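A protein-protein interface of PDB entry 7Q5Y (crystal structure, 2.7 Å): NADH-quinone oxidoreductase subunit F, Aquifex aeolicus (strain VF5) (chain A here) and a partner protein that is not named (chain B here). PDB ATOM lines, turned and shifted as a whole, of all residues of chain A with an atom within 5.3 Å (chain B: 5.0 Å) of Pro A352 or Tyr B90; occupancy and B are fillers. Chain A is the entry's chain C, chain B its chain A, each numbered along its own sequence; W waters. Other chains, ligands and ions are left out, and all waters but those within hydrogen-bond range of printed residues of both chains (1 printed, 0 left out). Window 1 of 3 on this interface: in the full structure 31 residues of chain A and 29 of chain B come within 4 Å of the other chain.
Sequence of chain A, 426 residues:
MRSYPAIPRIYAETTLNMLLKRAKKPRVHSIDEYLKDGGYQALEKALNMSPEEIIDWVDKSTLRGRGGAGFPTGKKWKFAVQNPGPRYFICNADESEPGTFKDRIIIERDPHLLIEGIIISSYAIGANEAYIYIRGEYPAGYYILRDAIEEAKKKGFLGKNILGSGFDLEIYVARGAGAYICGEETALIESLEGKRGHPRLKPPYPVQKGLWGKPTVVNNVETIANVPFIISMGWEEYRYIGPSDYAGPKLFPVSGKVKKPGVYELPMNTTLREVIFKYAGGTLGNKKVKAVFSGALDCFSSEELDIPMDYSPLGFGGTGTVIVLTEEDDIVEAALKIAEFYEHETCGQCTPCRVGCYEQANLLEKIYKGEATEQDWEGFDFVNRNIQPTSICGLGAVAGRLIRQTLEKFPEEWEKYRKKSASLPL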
ATOM      1  N   CYS A 350      34.515  30.103 -17.969  1.00  0.00           N
ATOM      2  CA  CYS A 350      34.014  29.800 -19.317  1.00  0.00           C
ATOM      3  C   CYS A 350      32.765  28.900 -19.350  1.00  0.00           C
ATOM      4  O   CYS A 350      32.584  27.990 -18.532  1.00  0.00           O
ATOM      5  CB  CYS A 350      35.133  29.227 -20.191  1.00  0.00           C
ATOM      6  SG  CYS A 350      35.843  27.654 -19.780  1.00  0.00           S
ATOM      7  N   THR A 351      31.908  29.177 -20.304  1.00  0.00           N
ATOM      8  CA  THR A 351      30.599  28.564 -20.507  1.00  0.00           C
ATOM      9  C   THR A 351      30.560  27.050 -20.515  1.00  0.00           C
ATOM     10  O   THR A 351      29.773  26.473 -19.767  1.00  0.00           O
ATOM     11  CB  THR A 351      29.984  29.049 -21.831  1.00  0.00           C
ATOM     12  OG1 THR A 351      30.032  30.470 -21.889  1.00  0.00           O
ATOM     13  CG2 THR A 351      28.565  28.615 -21.972  1.00  0.00           C
ATOM     14  N   PRO A 352      31.343  26.377 -21.366  1.00  0.00           N
ATOM     15  CA  PRO A 352      31.228  24.914 -21.435  1.00  0.00           C
ATOM     16  C   PRO A 352      31.421  24.218 -20.112  1.00  0.00           C
ATOM     17  O   PRO A 352      30.759  23.216 -19.832  1.00  0.00           O
ATOM     18  CB  PRO A 352      32.334  24.532 -22.427  1.00  0.00           C
ATOM     19  CG  PRO A 352      33.337  25.575 -22.260  1.00  0.00           C
ATOM     20  CD  PRO A 352      32.564  26.841 -22.058  1.00  0.00           C
ATOM     21  N   CYS A 353      32.305  24.731 -19.288  1.00  0.00           N
ATOM     22  CA  CYS A 353      32.586  24.108 -18.012  1.00  0.00           C
ATOM     23  C   CYS A 353      31.708  24.660 -16.893  1.00  0.00           C
ATOM     24  O   CYS A 353      31.212  23.888 -16.071  1.00  0.00           O
ATOM     25  CB  CYS A 353      34.084  24.265 -17.725  1.00  0.00           C
ATOM     26  SG  CYS A 353      34.624  23.799 -16.134  1.00  0.00           S
ATOM     27  N   ARG A 354      31.493  25.979 -16.845  1.00  0.00           N
ATOM     28  CA  ARG A 354      30.612  26.544 -15.830  1.00  0.00           C
ATOM     29  C   ARG A 354      29.260  25.833 -15.837  1.00  0.00           C
ATOM     30  O   ARG A 354      28.767  25.403 -14.790  1.00  0.00           O
ATOM     31  CB  ARG A 354      30.418  28.042 -16.088  1.00  0.00           C
ATOM     32  CG  ARG A 354      29.673  28.843 -15.002  1.00  0.00           C
ATOM     33  CD  ARG A 354      29.079  30.161 -15.597  1.00  0.00           C
ATOM     34  NE  ARG A 354      27.604  30.108 -15.674  1.00  0.00           N
ATOM     35  CZ  ARG A 354      26.922  30.394 -16.780  1.00  0.00           C
ATOM     36  NH1 ARG A 354      27.598  30.771 -17.879  1.00  0.00           N
ATOM     37  NH2 ARG A 354      25.578  30.336 -16.791  1.00  0.00           N
ATOM     38  N   VAL A 355      28.669  25.658 -17.024  1.00  0.00           N
ATOM     39  CA  VAL A 355      27.361  25.011 -17.148  1.00  0.00           C
ATOM     40  C   VAL A 355      27.466  23.508 -17.313  1.00  0.00           C
ATOM     41  O   VAL A 355      26.670  22.767 -16.726  1.00  0.00           O
ATOM     42  CB  VAL A 355      26.576  25.641 -18.311  1.00  0.00           C
ATOM     43  CG1 VAL A 355      25.227  24.978 -18.426  1.00  0.00           C
ATOM     44  CG2 VAL A 355      26.434  27.171 -18.123  1.00  0.00           C
ATOM     45  N   GLY A 356      28.439  23.037 -18.099  1.00  0.00           N
ATOM     46  CA  GLY A 356      28.578  21.601 -18.311  1.00  0.00           C
ATOM     47  C   GLY A 356      28.732  20.814 -17.020  1.00  0.00           C
ATOM     48  O   GLY A 356      28.047  19.809 -16.804  1.00  0.00           O
ATOM     49  N   CYS A 357      29.639  21.257 -16.139  1.00  0.00           N
ATOM     50  CA  CYS A 357      29.859  20.525 -14.893  1.00  0.00           C
ATOM     51  C   CYS A 357      28.613  20.495 -14.033  1.00  0.00           C
ATOM     52  O   CYS A 357      28.316  19.477 -13.396  1.00  0.00           O
ATOM     53  CB  CYS A 357      31.011  21.127 -14.097  1.00  0.00           C
ATOM     54  SG  CYS A 357      32.633  21.005 -14.903  1.00  0.00           S
ATOM     55  N   PHE A 382      24.884  14.503 -24.292  1.00  0.00           N
ATOM     56  CA  PHE A 382      25.232  15.742 -24.978  1.00  0.00           C
ATOM     57  C   PHE A 382      26.184  16.598 -24.160  1.00  0.00           C
ATOM     58  O   PHE A 382      27.177  17.117 -24.682  1.00  0.00           O
ATOM     59  CB  PHE A 382      23.952  16.521 -25.276  1.00  0.00           C
ATOM     60  CG  PHE A 382      24.146  17.738 -26.138  1.00  0.00           C
ATOM     61  CD1 PHE A 382      24.635  17.625 -27.432  1.00  0.00           C
ATOM     62  CD2 PHE A 382      23.848  19.008 -25.647  1.00  0.00           C
ATOM     63  CE1 PHE A 382      24.798  18.757 -28.240  1.00  0.00           C
ATOM     64  CE2 PHE A 382      24.010  20.139 -26.454  1.00  0.00           C
ATOM     65  CZ  PHE A 382      24.489  20.011 -27.751  1.00  0.00           C
ATOM     66  N   VAL A 383      25.877  16.783 -22.879  1.00  0.00           N
ATOM     67  CA  VAL A 383      26.720  17.610 -22.021  1.00  0.00           C
ATOM     68  C   VAL A 383      28.067  16.945 -21.789  1.00  0.00           C
ATOM     69  O   VAL A 383      29.124  17.541 -22.020  1.00  0.00           O
ATOM     70  CB  VAL A 383      26.007  17.904 -20.689  1.00  0.00           C
ATOM     71  CG1 VAL A 383      26.944  18.633 -19.739  1.00  0.00           C
ATOM     72  CG2 VAL A 383      24.715  18.680 -20.917  1.00  0.00           C
ATOM     73  N   ASN A 386      30.559  17.398 -24.537  1.00  0.00           N
ATOM     74  CA  ASN A 386      30.865  18.728 -25.074  1.00  0.00           C
ATOM     75  C   ASN A 386      31.470  19.738 -24.091  1.00  0.00           C
ATOM     76  O   ASN A 386      31.645  20.917 -24.449  1.00  0.00           O
ATOM     77  CB  ASN A 386      29.608  19.303 -25.710  1.00  0.00           C
ATOM     78  CG  ASN A 386      29.387  18.757 -27.070  1.00  0.00           C
ATOM     79  OD1 ASN A 386      30.292  18.807 -27.892  1.00  0.00           O
ATOM     80  ND2 ASN A 386      28.213  18.167 -27.312  1.00  0.00           N
ATOM     81  N   ILE A 387      31.802  19.324 -22.872  1.00  0.00           N
ATOM     82  CA  ILE A 387      32.421  20.242 -21.922  1.00  0.00           C
ATOM     83  C   ILE A 387      33.852  20.548 -22.334  1.00  0.00           C
ATOM     84  O   ILE A 387      34.323  21.682 -22.230  1.00  0.00           O
ATOM     85  CB  ILE A 387      32.406  19.613 -20.516  1.00  0.00           C
ATOM     86  CG1 ILE A 387      30.995  19.294 -20.042  1.00  0.00           C
ATOM     87  CG2 ILE A 387      33.214  20.432 -19.515  1.00  0.00           C
ATOM     88  CD1 ILE A 387      31.019  18.491 -18.769  1.00  0.00           C
ATOM     89  N   THR A 390      35.678  23.357 -25.955  1.00  0.00           N
ATOM     90  CA  THR A 390      36.016  24.773 -25.855  1.00  0.00           C
ATOM     91  C   THR A 390      36.450  25.214 -24.460  1.00  0.00           C
ATOM     92  O   THR A 390      36.729  26.397 -24.273  1.00  0.00           O
ATOM     93  CB  THR A 390      34.849  25.649 -26.311  1.00  0.00           C
ATOM     94  OG1 THR A 390      33.728  25.415 -25.452  1.00  0.00           O
ATOM     95  CG2 THR A 390      34.456  25.305 -27.747  1.00  0.00           C
ATOM     96  N   SER A 391      36.542  24.315 -23.481  1.00  0.00           N
ATOM     97  CA  SER A 391      36.992  24.737 -22.161  1.00  0.00           C
ATOM     98  C   SER A 391      38.335  25.446 -22.270  1.00  0.00           C
ATOM     99  O   SER A 391      39.114  25.206 -23.201  1.00  0.00           O
ATOM    100  CB  SER A 391      37.107  23.551 -21.215  1.00  0.00           C
ATOM    101  OG  SER A 391      35.831  23.134 -20.794  1.00  0.00           O
ATOM    102  N   CYS B  48      33.306  33.741 -22.872  1.00  0.00           N
ATOM    103  CA  CYS B  48      32.068  33.140 -23.354  1.00  0.00           C
ATOM    104  C   CYS B  48      32.324  31.957 -24.278  1.00  0.00           C
ATOM    105  O   CYS B  48      31.530  31.009 -24.286  1.00  0.00           O
ATOM    106  CB  CYS B  48      31.189  34.211 -24.019  1.00  0.00           C
ATOM    107  SG  CYS B  48      31.425  34.489 -25.766  1.00  0.00           S
ATOM    108  N   ARG B  49      33.410  31.989 -25.057  1.00  0.00           N
ATOM    109  CA  ARG B  49      33.820  30.938 -25.991  1.00  0.00           C
ATOM    110  C   ARG B  49      32.864  30.781 -27.161  1.00  0.00           C
ATOM    111  O   ARG B  49      33.058  29.888 -27.966  1.00  0.00           O
ATOM    112  CB  ARG B  49      33.960  29.571 -25.308  1.00  0.00           C
ATOM    113  CG  ARG B  49      34.701  29.614 -23.984  1.00  0.00           C
ATOM    114  CD  ARG B  49      36.103  29.090 -24.131  1.00  0.00           C
ATOM    115  NE  ARG B  49      37.177  30.065 -24.228  1.00  0.00           N
ATOM    116  CZ  ARG B  49      38.386  29.756 -24.667  1.00  0.00           C
ATOM    117  NH1 ARG B  49      38.657  28.525 -25.043  1.00  0.00           N
ATOM    118  NH2 ARG B  49      39.322  30.673 -24.727  1.00  0.00           N
ATOM    119  N   GLU B  86      28.626  22.302 -34.036  1.00  0.00           N
ATOM    120  CA  GLU B  86      28.232  21.527 -32.864  1.00  0.00           C
ATOM    121  C   GLU B  86      28.543  22.273 -31.579  1.00  0.00           C
ATOM    122  O   GLU B  86      27.753  22.234 -30.627  1.00  0.00           O
ATOM    123  CB  GLU B  86      28.877  20.143 -32.868  1.00  0.00           C
ATOM    124  CG  GLU B  86      27.995  19.095 -33.545  1.00  0.00           C
ATOM    125  CD  GLU B  86      28.787  17.953 -34.183  1.00  0.00           C
ATOM    126  OE1 GLU B  86      30.017  17.868 -33.936  1.00  0.00           O
ATOM    127  OE2 GLU B  86      28.180  17.138 -34.928  1.00  0.00           O
ATOM    128  N   GLN B  87      29.670  22.982 -31.533  1.00  0.00           N
ATOM    129  CA  GLN B  87      29.986  23.714 -30.319  1.00  0.00           C
ATOM    130  C   GLN B  87      29.051  24.905 -30.129  1.00  0.00           C
ATOM    131  O   GLN B  87      28.699  25.239 -28.990  1.00  0.00           O
ATOM    132  CB  GLN B  87      31.444  24.142 -30.338  1.00  0.00           C
ATOM    133  CG  GLN B  87      32.394  23.003 -30.083  1.00  0.00           C
ATOM    134  CD  GLN B  87      31.921  22.120 -28.950  1.00  0.00           C
ATOM    135  OE1 GLN B  87      31.813  22.554 -27.790  1.00  0.00           O
ATOM    136  NE2 GLN B  87      31.688  20.867 -29.261  1.00  0.00           N
ATOM    137  N   GLN B  88      28.617  25.544 -31.219  1.00  0.00           N
ATOM    138  CA  GLN B  88      27.673  26.643 -31.067  1.00  0.00           C
ATOM    139  C   GLN B  88      26.371  26.128 -30.476  1.00  0.00           C
ATOM    140  O   GLN B  88      25.802  26.746 -29.567  1.00  0.00           O
ATOM    141  CB  GLN B  88      27.443  27.337 -32.405  1.00  0.00           C
ATOM    142  CG  GLN B  88      28.584  28.248 -32.793  1.00  0.00           C
ATOM    143  CD  GLN B  88      28.525  28.682 -34.246  1.00  0.00           C
ATOM    144  OE1 GLN B  88      27.606  28.313 -34.994  1.00  0.00           O
ATOM    145  NE2 GLN B  88      29.526  29.458 -34.659  1.00  0.00           N
ATOM    146  N   LYS B  89      25.888  24.986 -30.970  1.00  0.00           N
ATOM    147  CA  LYS B  89      24.655  24.429 -30.419  1.00  0.00           C
ATOM    148  C   LYS B  89      24.857  24.052 -28.955  1.00  0.00           C
ATOM    149  O   LYS B  89      23.977  24.282 -28.119  1.00  0.00           O
ATOM    150  CB  LYS B  89      24.202  23.222 -31.243  1.00  0.00           C
ATOM    151  CG  LYS B  89      23.876  23.603 -32.684  1.00  0.00           C
ATOM    152  CD  LYS B  89      23.182  22.506 -33.503  1.00  0.00           C
ATOM    153  CE  LYS B  89      22.818  23.041 -34.901  1.00  0.00           C
ATOM    154  NZ  LYS B  89      21.863  22.185 -35.666  1.00  0.00           N
ATOM    155  N   TYR B  90      26.024  23.502 -28.611  1.00  0.00           N
ATOM    156  CA  TYR B  90      26.224  23.134 -27.217  1.00  0.00           C
ATOM    157  C   TYR B  90      26.322  24.369 -26.330  1.00  0.00           C
ATOM    158  O   TYR B  90      25.686  24.436 -25.273  1.00  0.00           O
ATOM    159  CB  TYR B  90      27.465  22.273 -27.039  1.00  0.00           C
ATOM    160  CG  TYR B  90      27.819  22.191 -25.574  1.00  0.00           C
ATOM    161  CD1 TYR B  90      27.015  21.504 -24.685  1.00  0.00           C
ATOM    162  CD2 TYR B  90      28.922  22.859 -25.065  1.00  0.00           C
ATOM    163  CE1 TYR B  90      27.322  21.452 -23.342  1.00  0.00           C
ATOM    164  CE2 TYR B  90      29.223  22.825 -23.716  1.00  0.00           C
ATOM    165  CZ  TYR B  90      28.425  22.116 -22.863  1.00  0.00           C
ATOM    166  OH  TYR B  90      28.732  22.062 -21.521  1.00  0.00           O
ATOM    167  N   LEU B  91      27.130  25.350 -26.732  1.00  0.00           N
ATOM    168  CA  LEU B  91      27.287  26.560 -25.924  1.00  0.00           C
ATOM    169  C   LEU B  91      25.952  27.289 -25.739  1.00  0.00           C
ATOM    170  O   LEU B  91      25.617  27.725 -24.632  1.00  0.00           O
ATOM    171  CB  LEU B  91      28.346  27.470 -26.554  1.00  0.00           C
ATOM    172  CG  LEU B  91      29.816  27.025 -26.485  1.00  0.00           C
ATOM    173  CD1 LEU B  91      30.715  28.023 -27.207  1.00  0.00           C
ATOM    174  CD2 LEU B  91      30.292  26.796 -25.038  1.00  0.00           C
ATOM    175  N   LEU B  92      25.177  27.445 -26.814  1.00  0.00           N
ATOM    176  CA  LEU B  92      23.892  28.119 -26.665  1.00  0.00           C
ATOM    177  C   LEU B  92      22.942  27.294 -25.805  1.00  0.00           C
ATOM    178  O   LEU B  92      22.199  27.851 -24.990  1.00  0.00           O
ATOM    179  CB  LEU B  92      23.295  28.447 -28.027  1.00  0.00           C
ATOM    180  CG  LEU B  92      24.153  29.549 -28.670  1.00  0.00           C
ATOM    181  CD1 LEU B  92      23.985  29.678 -30.175  1.00  0.00           C
ATOM    182  CD2 LEU B  92      23.874  30.850 -28.011  1.00  0.00           C
ATOM    183  N   GLN B  93      22.967  25.966 -25.941  1.00  0.00           N
ATOM    184  CA  GLN B  93      22.103  25.151 -25.089  1.00  0.00           C
ATOM    185  C   GLN B  93      22.509  25.279 -23.625  1.00  0.00           C
ATOM    186  O   GLN B  93      21.653  25.296 -22.724  1.00  0.00           O
ATOM    187  CB  GLN B  93      22.154  23.686 -25.507  1.00  0.00           C
ATOM    188  CG  GLN B  93      21.571  22.751 -24.456  1.00  0.00           C
ATOM    189  CD  GLN B  93      20.072  22.871 -24.327  1.00  0.00           C
ATOM    190  OE1 GLN B  93      19.334  22.038 -24.836  1.00  0.00           O
ATOM    191  NE2 GLN B  93      19.617  23.899 -23.646  1.00  0.00           N
ATOM    192  N   ALA B  94      23.818  25.358 -23.374  1.00  0.00           N
ATOM    193  CA  ALA B  94      24.307  25.502 -22.011  1.00  0.00           C
ATOM    194  C   ALA B  94      23.810  26.803 -21.414  1.00  0.00           C
ATOM    195  O   ALA B  94      23.359  26.847 -20.259  1.00  0.00           O
ATOM    196  CB  ALA B  94      25.836  25.422 -21.976  1.00  0.00           C
ATOM    197  N   LEU B  95      23.895  27.886 -22.182  1.00  0.00           N
ATOM    198  CA  LEU B  95      23.403  29.144 -21.645  1.00  0.00           C
ATOM    199  C   LEU B  95      21.914  29.048 -21.325  1.00  0.00           C
ATOM    200  O   LEU B  95      21.465  29.544 -20.291  1.00  0.00           O
ATOM    201  CB  LEU B  95      23.716  30.297 -22.607  1.00  0.00           C
ATOM    202  CG  LEU B  95      25.220  30.638 -22.699  1.00  0.00           C
ATOM    203  CD1 LEU B  95      25.551  31.716 -23.724  1.00  0.00           C
ATOM    204  CD2 LEU B  95      25.694  31.077 -21.367  1.00  0.00           C
HETATM  205  O   HOH W   1      39.388  25.455 -26.271  1.00  0.00           O
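Of the printed residues of chain B, Pro A352 touches Arg B49, Tyr B90 and Leu B91. Of the printed residues of chain B, Ser A391 touches Arg B49. Printed residues of chain A within 4 Å of Arg B49: Cys A350, Pro A352, Thr A390 and Ser A391. Of the printed residues of chain A, Gln B87 touches Asn A386 (2.8 Å) and Thr A390 (3.8 Å). Gln B88 touches none of the printed residues of chain A. Tyr B90 touches just these residues of chain A: Pro A352, Gly A356, Phe A382, Asn A386 and Ile A387. Printed residues of chain A within 4 Å of Leu B95: Thr A351 (3.8 Å) and Arg A354 (3.99 Å). The nearest printed residue of chain B that does not touch Pro A352 is Cys B48 (4.8 Å). The nearest printed residue of chain B that does not touch Ile A387 is Gln B87 (5.9 Å).
The backbone carbonyl oxygen of Cys B48 is in hydrogen-bond range of the side-chain hydroxyl of Thr A351. OD1 of Asn A386 is in hydrogen-bond range of NE2 of Gln B87 (2.8 Å). The side-chain hydroxyl (OH) of Tyr B90 lies within hydrogen-bond range of the backbone carbonyl oxygen (O) of Pro A352 (2.9 Å). The backbone carbonyl oxygen of Thr A390 sits close to the guanidinium group of Arg B49 (3.0 Å).
Of the 12 printed residues of chain B, 7 touch a printed residue of chain A. Among the printed residues, 18 pairs touch across the chains. Among the printed residues, no Asp or Glu carboxylate lies within 4 Å of a Lys or Arg side-chain nitrogen of the other chain.
The side-chain hydroxyl (OG) of Ser A391 lies within hydrogen-bond range of the backbone carbonyl oxygen (O) of Ile A387. ND2 of Asn A386 sits at hydrogen-bond distance from O of Phe A382 (3.0 Å).
Among the printed residues, pairs that only touch across the chains: Cys A350 with Arg B49 (3.8 Å), Thr A351 with Leu B91 (3.9 Å), Thr A351 with Leu B95 (3.8 Å), Pro A352 with Arg B49 (3.996 Å), Pro A352 with Leu B91 (3.7 Å), Arg A354 with Leu B95 (3.99 Å), Val A355 with Ala B94 (3.2 Å), Gly A356 with Tyr B90 (3.2 Å), Phe A382 with Tyr B90 (3.6 Å), Asn A386 with Tyr B90 (3.2 Å), Ile A387 with Tyr B90 (3.9 Å), Thr A390 with Gln B87 (3.8 Å), Thr A390 with Leu B91 (3.7 Å) and Ser A391 with Arg B49 (3.8 Å).
Water W1 lies within hydrogen-bond range of the backbone carbonyl oxygen (O) of Ser A391 (3.1 Å), the guanidinium group (NH1) of Arg B49 (3.4 Å) and the backbone carbonyl oxygen (O) of Thr A390 (3.5 Å).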
